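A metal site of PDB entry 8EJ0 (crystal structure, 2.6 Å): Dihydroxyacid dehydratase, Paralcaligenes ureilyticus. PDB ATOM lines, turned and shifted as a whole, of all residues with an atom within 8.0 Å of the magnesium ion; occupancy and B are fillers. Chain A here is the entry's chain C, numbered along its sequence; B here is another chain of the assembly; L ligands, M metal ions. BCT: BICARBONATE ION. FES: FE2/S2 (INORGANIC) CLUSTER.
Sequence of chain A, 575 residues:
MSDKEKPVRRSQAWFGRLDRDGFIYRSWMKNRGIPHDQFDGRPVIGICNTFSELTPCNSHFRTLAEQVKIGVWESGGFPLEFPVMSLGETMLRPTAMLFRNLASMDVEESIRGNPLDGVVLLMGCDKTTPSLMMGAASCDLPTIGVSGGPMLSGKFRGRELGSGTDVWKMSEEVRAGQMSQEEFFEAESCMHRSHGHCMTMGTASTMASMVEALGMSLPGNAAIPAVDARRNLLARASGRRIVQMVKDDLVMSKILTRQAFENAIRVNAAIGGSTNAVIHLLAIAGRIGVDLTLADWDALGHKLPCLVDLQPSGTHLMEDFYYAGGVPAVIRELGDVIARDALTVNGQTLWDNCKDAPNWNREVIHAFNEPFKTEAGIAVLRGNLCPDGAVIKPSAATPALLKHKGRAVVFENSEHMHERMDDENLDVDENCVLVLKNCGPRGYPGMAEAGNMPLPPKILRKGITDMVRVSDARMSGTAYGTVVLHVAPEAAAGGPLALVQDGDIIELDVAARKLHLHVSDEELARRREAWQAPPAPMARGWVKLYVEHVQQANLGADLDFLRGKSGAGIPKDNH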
ATOM      1  N   GLU A  89      19.106  13.049  -6.496  1.00  0.00           N
ATOM      2  CA  GLU A  89      18.518  13.283  -5.183  1.00  0.00           C
ATOM      3  C   GLU A  89      19.052  14.562  -4.541  1.00  0.00           C
ATOM      4  O   GLU A  89      18.288  15.327  -3.936  1.00  0.00           O
ATOM      5  CB  GLU A  89      18.766  12.086  -4.273  1.00  0.00           C
ATOM      6  CG  GLU A  89      18.290  12.275  -2.852  1.00  0.00           C
ATOM      7  CD  GLU A  89      17.419  11.145  -2.382  1.00  0.00           C
ATOM      8  OE1 GLU A  89      16.421  10.835  -3.072  1.00  0.00           O
ATOM      9  OE2 GLU A  89      17.739  10.538  -1.338  1.00  0.00           O
ATOM     10  N   THR A  90      20.361  14.802  -4.646  1.00  0.00           N
ATOM     11  CA  THR A  90      20.936  15.991  -4.023  1.00  0.00           C
ATOM     12  C   THR A  90      20.523  17.281  -4.731  1.00  0.00           C
ATOM     13  O   THR A  90      20.650  18.355  -4.136  1.00  0.00           O
ATOM     14  CB  THR A  90      22.461  15.886  -3.998  1.00  0.00           C
ATOM     15  OG1 THR A  90      22.959  15.709  -5.335  1.00  0.00           O
ATOM     16  CG2 THR A  90      22.910  14.715  -3.144  1.00  0.00           C
ATOM     17  N   THR A  95      12.094  17.877  -3.201  1.00  0.00           N
ATOM     18  CA  THR A  95      12.646  16.543  -2.973  1.00  0.00           C
ATOM     19  C   THR A  95      12.501  15.718  -4.239  1.00  0.00           C
ATOM     20  O   THR A  95      11.586  15.939  -5.028  1.00  0.00           O
ATOM     21  CB  THR A  95      11.948  15.848  -1.798  1.00  0.00           C
ATOM     22  OG1 THR A  95      12.394  14.491  -1.711  1.00  0.00           O
ATOM     23  CG2 THR A  95      10.436  15.866  -1.984  1.00  0.00           C
ATOM     24  N   ALA A  96      13.423  14.767  -4.429  1.00  0.00           N
ATOM     25  CA  ALA A  96      13.364  13.917  -5.617  1.00  0.00           C
ATOM     26  C   ALA A  96      12.147  13.001  -5.592  1.00  0.00           C
ATOM     27  O   ALA A  96      11.640  12.619  -6.653  1.00  0.00           O
ATOM     28  CB  ALA A  96      14.644  13.096  -5.744  1.00  0.00           C
ATOM     29  N   MET A  97      11.670  12.639  -4.404  1.00  0.00           N
ATOM     30  CA  MET A  97      10.478  11.792  -4.297  1.00  0.00           C
ATOM     31  C   MET A  97       9.261  12.449  -4.929  1.00  0.00           C
ATOM     32  O   MET A  97       8.378  11.754  -5.439  1.00  0.00           O
ATOM     33  CB  MET A  97      10.209  11.454  -2.833  1.00  0.00           C
ATOM     34  CG  MET A  97       8.828  10.865  -2.556  1.00  0.00           C
ATOM     35  SD  MET A  97       8.564   9.239  -3.279  1.00  0.00           S
ATOM     36  CE  MET A  97       9.297   8.208  -2.010  1.00  0.00           C
ATOM     37  N   CYS A 125      20.916   6.703  -9.051  1.00  0.00           N
ATOM     38  CA  CYS A 125      20.580   7.313  -7.775  1.00  0.00           C
ATOM     39  C   CYS A 125      19.202   6.880  -7.325  1.00  0.00           C
ATOM     40  O   CYS A 125      18.373   6.449  -8.132  1.00  0.00           O
ATOM     41  CB  CYS A 125      20.656   8.839  -7.892  1.00  0.00           C
ATOM     42  SG  CYS A 125      20.609   9.738  -6.324  1.00  0.00           S
ATOM     43  N   ASP A 126      18.956   6.991  -6.021  1.00  0.00           N
ATOM     44  CA  ASP A 126      17.789   6.413  -5.340  1.00  0.00           C
ATOM     45  C   ASP A 126      16.523   6.358  -6.174  1.00  0.00           C
ATOM     46  O   ASP A 126      16.119   5.292  -6.643  1.00  0.00           O
ATOM     47  CB  ASP A 126      17.481   7.191  -4.054  1.00  0.00           C
ATOM     48  CG  ASP A 126      18.731   7.618  -3.322  1.00  0.00           C
ATOM     49  OD1 ASP A 126      19.043   8.838  -3.324  1.00  0.00           O
ATOM     50  OD2 ASP A 126      19.417   6.747  -2.758  1.00  0.00           O
ATOM     51  N   KCX A 127      15.914   7.531  -6.384  1.00  0.00           N
ATOM     52  CA  KCX A 127      14.614   7.649  -7.010  1.00  0.00           C
ATOM     53  CB  KCX A 127      14.216   9.127  -7.015  1.00  0.00           C
ATOM     54  CG  KCX A 127      12.977   9.404  -6.180  1.00  0.00           C
ATOM     55  CD  KCX A 127      12.970   8.640  -4.859  1.00  0.00           C
ATOM     56  CE  KCX A 127      13.528   9.469  -3.703  1.00  0.00           C
ATOM     57  NZ  KCX A 127      13.320   8.765  -2.441  1.00  0.00           N
ATOM     58  C   KCX A 127      14.542   7.085  -8.446  1.00  0.00           C
ATOM     59  O   KCX A 127      13.496   6.800  -8.904  1.00  0.00           O
ATOM     60  CX  KCX A 127      14.431   8.096  -1.802  1.00  0.00           C
ATOM     61  OQ1 KCX A 127      14.228   7.071  -1.098  1.00  0.00           O
ATOM     62  OQ2 KCX A 127      15.607   8.518  -1.934  1.00  0.00           O
ATOM     63  N   TRP A 168      25.539  13.951   8.080  1.00  0.00           N
ATOM     64  CA  TRP A 168      24.821  14.191   9.329  1.00  0.00           C
ATOM     65  C   TRP A 168      25.777  14.210  10.515  1.00  0.00           C
ATOM     66  O   TRP A 168      25.628  15.036  11.427  1.00  0.00           O
ATOM     67  CB  TRP A 168      23.751  13.122   9.549  1.00  0.00           C
ATOM     68  CG  TRP A 168      23.133  12.559   8.294  1.00  0.00           C
ATOM     69  CD1 TRP A 168      23.135  11.256   7.904  1.00  0.00           C
ATOM     70  CD2 TRP A 168      22.419  13.286   7.288  1.00  0.00           C
ATOM     71  NE1 TRP A 168      22.472  11.126   6.708  1.00  0.00           N
ATOM     72  CE2 TRP A 168      22.030  12.350   6.306  1.00  0.00           C
ATOM     73  CE3 TRP A 168      22.084  14.629   7.103  1.00  0.00           C
ATOM     74  CZ2 TRP A 168      21.306  12.714   5.168  1.00  0.00           C
ATOM     75  CZ3 TRP A 168      21.370  14.991   5.979  1.00  0.00           C
ATOM     76  CH2 TRP A 168      20.987  14.040   5.025  1.00  0.00           C
ATOM     77  N   CYS A 198      25.484   6.925  -3.812  1.00  0.00           N
ATOM     78  CA  CYS A 198      25.886   7.005  -2.418  1.00  0.00           C
ATOM     79  C   CYS A 198      26.403   5.664  -1.913  1.00  0.00           C
ATOM     80  O   CYS A 198      25.689   4.660  -1.913  1.00  0.00           O
ATOM     81  CB  CYS A 198      24.720   7.463  -1.552  1.00  0.00           C
ATOM     82  SG  CYS A 198      24.710   9.256  -1.344  1.00  0.00           S
ATOM     83  N   GLY A 202      22.659   3.327   1.918  1.00  0.00           N
ATOM     84  CA  GLY A 202      21.548   4.239   1.697  1.00  0.00           C
ATOM     85  C   GLY A 202      20.532   3.658   0.738  1.00  0.00           C
ATOM     86  O   GLY A 202      20.550   2.470   0.401  1.00  0.00           O
ATOM     87  N   THR A 203      19.629   4.523   0.286  1.00  0.00           N
ATOM     88  CA  THR A 203      18.537   4.065  -0.564  1.00  0.00           C
ATOM     89  C   THR A 203      19.050   3.421  -1.846  1.00  0.00           C
ATOM     90  O   THR A 203      18.571   2.346  -2.245  1.00  0.00           O
ATOM     91  CB  THR A 203      17.597   5.224  -0.904  1.00  0.00           C
ATOM     92  OG1 THR A 203      17.127   5.827   0.309  1.00  0.00           O
ATOM     93  CG2 THR A 203      16.392   4.720  -1.697  1.00  0.00           C
ATOM     94  N   ALA A 204      20.040   4.033  -2.493  1.00  0.00           N
ATOM     95  CA  ALA A 204      20.548   3.500  -3.757  1.00  0.00           C
ATOM     96  C   ALA A 204      21.184   2.131  -3.569  1.00  0.00           C
ATOM     97  O   ALA A 204      21.008   1.236  -4.396  1.00  0.00           O
ATOM     98  CB  ALA A 204      21.539   4.475  -4.385  1.00  0.00           C
ATOM     99  N   SER A 274      17.592   0.547   3.936  1.00  0.00           N
ATOM    100  CA  SER A 274      16.988   1.853   4.153  1.00  0.00           C
ATOM    101  C   SER A 274      15.480   1.734   4.367  1.00  0.00           C
ATOM    102  O   SER A 274      14.827   0.834   3.828  1.00  0.00           O
ATOM    103  CB  SER A 274      17.261   2.755   2.950  1.00  0.00           C
ATOM    104  OG  SER A 274      16.404   3.889   2.951  1.00  0.00           O
ATOM    105  N   ASN A 276      13.389   3.777   3.150  1.00  0.00           N
ATOM    106  CA  ASN A 276      12.725   4.175   1.919  1.00  0.00           C
ATOM    107  C   ASN A 276      12.411   2.991   1.014  1.00  0.00           C
ATOM    108  O   ASN A 276      11.546   3.111   0.144  1.00  0.00           O
ATOM    109  CB  ASN A 276      13.582   5.186   1.169  1.00  0.00           C
ATOM    110  CG  ASN A 276      13.621   6.544   1.855  1.00  0.00           C
ATOM    111  OD1 ASN A 276      12.619   6.992   2.418  1.00  0.00           O
ATOM    112  ND2 ASN A 276      14.768   7.200   1.809  1.00  0.00           N
ATOM    113  N   HIS A 280       9.101   2.219  -1.495  1.00  0.00           N
ATOM    114  CA  HIS A 280       9.357   1.965  -2.916  1.00  0.00           C
ATOM    115  C   HIS A 280       8.870   0.587  -3.335  1.00  0.00           C
ATOM    116  O   HIS A 280       8.282   0.434  -4.410  1.00  0.00           O
ATOM    117  CB  HIS A 280      10.837   2.139  -3.209  1.00  0.00           C
ATOM    118  CG  HIS A 280      11.299   3.565  -3.166  1.00  0.00           C
ATOM    119  ND1 HIS A 280      10.509   4.616  -3.587  1.00  0.00           N
ATOM    120  CD2 HIS A 280      12.468   4.119  -2.764  1.00  0.00           C
ATOM    121  CE1 HIS A 280      11.169   5.752  -3.436  1.00  0.00           C
ATOM    122  NE2 HIS A 280      12.362   5.474  -2.941  1.00  0.00           N
ATOM    123  N   GLU A 449      13.178  14.025   2.896  1.00  0.00           N
ATOM    124  CA  GLU A 449      13.992  13.288   3.861  1.00  0.00           C
ATOM    125  C   GLU A 449      14.424  14.239   4.977  1.00  0.00           C
ATOM    126  O   GLU A 449      15.577  14.658   5.086  1.00  0.00           O
ATOM    127  CB  GLU A 449      15.188  12.653   3.169  1.00  0.00           C
ATOM    128  CG  GLU A 449      14.826  11.566   2.177  1.00  0.00           C
ATOM    129  CD  GLU A 449      16.005  11.120   1.339  1.00  0.00           C
ATOM    130  OE1 GLU A 449      17.158  11.423   1.727  1.00  0.00           O
ATOM    131  OE2 GLU A 449      15.784  10.463   0.294  1.00  0.00           O
ATOM    132  N   ARG A 474      10.077  11.254   5.462  1.00  0.00           N
ATOM    133  CA  ARG A 474      11.096  10.231   5.282  1.00  0.00           C
ATOM    134  C   ARG A 474      12.402  10.721   5.892  1.00  0.00           C
ATOM    135  O   ARG A 474      12.535  11.857   6.365  1.00  0.00           O
ATOM    136  CB  ARG A 474      11.272   9.900   3.799  1.00  0.00           C
ATOM    137  CG  ARG A 474      10.059   9.278   3.144  1.00  0.00           C
ATOM    138  CD  ARG A 474      10.274   9.068   1.644  1.00  0.00           C
ATOM    139  NE  ARG A 474      10.746  10.278   0.978  1.00  0.00           N
ATOM    140  CZ  ARG A 474      11.969  10.441   0.507  1.00  0.00           C
ATOM    141  NH1 ARG A 474      12.860   9.462   0.615  1.00  0.00           N
ATOM    142  NH2 ARG A 474      12.319  11.573  -0.094  1.00  0.00           N
ATOM    143  N   MET A 475      13.400   9.838   5.878  1.00  0.00           N
ATOM    144  CA  MET A 475      14.770  10.233   6.165  1.00  0.00           C
ATOM    145  C   MET A 475      15.679   9.498   5.192  1.00  0.00           C
ATOM    146  O   MET A 475      15.306   8.474   4.616  1.00  0.00           O
ATOM    147  CB  MET A 475      15.176   9.928   7.619  1.00  0.00           C
ATOM    148  CG  MET A 475      15.691   8.523   7.842  1.00  0.00           C
ATOM    149  SD  MET A 475      16.168   8.230   9.557  1.00  0.00           S
ATOM    150  CE  MET A 475      16.985   6.645   9.433  1.00  0.00           C
ATOM    151  N   SER A 476      16.877  10.052   5.008  1.00  0.00           N
ATOM    152  CA  SER A 476      17.846   9.407   4.131  1.00  0.00           C
ATOM    153  C   SER A 476      18.143   8.000   4.608  1.00  0.00           C
ATOM    154  O   SER A 476      18.211   7.731   5.811  1.00  0.00           O
ATOM    155  CB  SER A 476      19.136  10.233   4.082  1.00  0.00           C
ATOM    156  OG  SER A 476      20.147   9.554   3.362  1.00  0.00           O
ATOM    157  N   GLY A 477      18.310   7.074   3.650  1.00  0.00           N
ATOM    158  CA  GLY A 477      18.770   5.750   3.991  1.00  0.00           C
ATOM    159  C   GLY A 477      20.128   5.750   4.656  1.00  0.00           C
ATOM    160  O   GLY A 477      20.481   4.779   5.341  1.00  0.00           O
ATOM    161  N   THR A 478      20.899   6.817   4.477  1.00  0.00           N
ATOM    162  CA  THR A 478      22.194   6.991   5.124  1.00  0.00           C
ATOM    163  C   THR A 478      22.080   7.546   6.537  1.00  0.00           C
ATOM    164  O   THR A 478      23.109   7.681   7.212  1.00  0.00           O
ATOM    165  CB  THR A 478      23.065   7.923   4.276  1.00  0.00           C
ATOM    166  OG1 THR A 478      22.657   9.278   4.472  1.00  0.00           O
ATOM    167  CG2 THR A 478      22.922   7.586   2.799  1.00  0.00           C
ATOM    168  N   ASN B 574      15.872  19.848   0.468  1.00  0.00           N
ATOM    169  CA  ASN B 574      15.441  18.463   0.331  1.00  0.00           C
ATOM    170  C   ASN B 574      15.861  17.582   1.503  1.00  0.00           C
ATOM    171  O   ASN B 574      15.674  16.368   1.441  1.00  0.00           O
ATOM    172  CB  ASN B 574      15.978  17.878  -0.987  1.00  0.00           C
ATOM    173  CG  ASN B 574      17.428  18.234  -1.229  1.00  0.00           C
ATOM    174  OD1 ASN B 574      18.173  18.528  -0.306  1.00  0.00           O
ATOM    175  ND2 ASN B 574      17.828  18.212  -2.500  1.00  0.00           N
ATOM    176  N   HIS B 575      16.405  18.172   2.558  1.00  0.00           N
ATOM    177  CA  HIS B 575      16.810  17.403   3.734  1.00  0.00           C
ATOM    178  C   HIS B 575      16.588  18.198   5.013  1.00  0.00           C
ATOM    179  O   HIS B 575      16.364  19.403   4.988  1.00  0.00           O
ATOM    180  CB  HIS B 575      18.271  16.969   3.619  1.00  0.00           C
ATOM    181  CG  HIS B 575      18.538  16.023   2.499  1.00  0.00           C
ATOM    182  ND1 HIS B 575      18.723  16.449   1.194  1.00  0.00           N
ATOM    183  CD2 HIS B 575      18.657  14.667   2.471  1.00  0.00           C
ATOM    184  CE1 HIS B 575      18.932  15.402   0.423  1.00  0.00           C
ATOM    185  NE2 HIS B 575      18.898  14.310   1.173  1.00  0.00           N
HETATM  186  C   BCT L   1      19.445   8.155   0.721  1.00  0.00           C
HETATM  187  O1  BCT L   1      20.059   6.960   0.953  1.00  0.00           O
HETATM  188  O2  BCT L   1      18.112   8.311   1.021  1.00  0.00           O
HETATM  189  O3  BCT L   1      20.115   9.133   0.409  1.00  0.00           O
HETATM  190 FE1  FES L   2      22.726   9.520  -5.649  1.00  0.00          FE
HETATM  191 FE2  FES L   2      22.727   9.234  -2.529  1.00  0.00          FE
HETATM  192  S1  FES L   2      22.357   7.941  -4.252  1.00  0.00           S
HETATM  193  S2  FES L   2      22.553  10.857  -3.966  1.00  0.00           S
HETATM  194 MG    MG M   1      17.294   9.094  -0.454  1.00  0.00          MG
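The side-chain sulfur of Cys 125 lies close to the backbone NH of Glu 89 (3.6 Å).
The backbone carbonyl oxygen (O) of Glu 89 is in hydrogen-bond range of the side-chain amide nitrogen (ND2) of Asn 574 of chain B.
OE2 of Glu 449 lies close to NH1 of Arg 474, at 3.1 Å.
OQ1 of KCX 127 lies within hydrogen-bond range of the side-chain amide nitrogen of Asn 276 (3.0 Å).
OQ1 of KCX 127 is in salt-bridge range of the guanidinium group (NH1) of Arg 474, 3.2 Å away.
OG of Ser 274 sits at hydrogen-bond distance from OG1 of Thr 203, at 3.4 Å.
The side-chain carboxylate (OD1) of Asp 126 lies close to the side-chain sulfur (SG) of Cys 125 (3.5 Å).
OD1 of Asn 276 sits at hydrogen-bond distance from NH1 of Arg 474 (3.1 Å).
The side-chain sulfur (SG) of Cys 125 binds an iron atom (FE1) of FES L2 (2.2 Å).
The backbone NH of Cys 198 lies close to a sulfur (S1) of FES L2.
An iron atom (FE2) of FES L2 is bound by the side-chain sulfur (SG) of Cys 198 (2.3 Å).
Asp 126 touches the magnesium ion (OD1 to MG, 3.4 Å).
OG1 of Thr 203 touches the magnesium ion, 3.4 Å away.
ND2 of Asn 276 touches the magnesium ion, 3.9 Å away.
The nearest printed residue that does not touch the magnesium ion is Arg 474 (4.6 Å).
The magnesium ion is bound by OE2 of Glu 89 (1.8 Å).
O2 of BCT L1 binds the magnesium ion (1.9 Å).
OE2 of Glu 449 is bound to the magnesium ion, 2.2 Å away.
OQ2 of KCX 127 is bound to the magnesium ion, at 2.3 Å.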
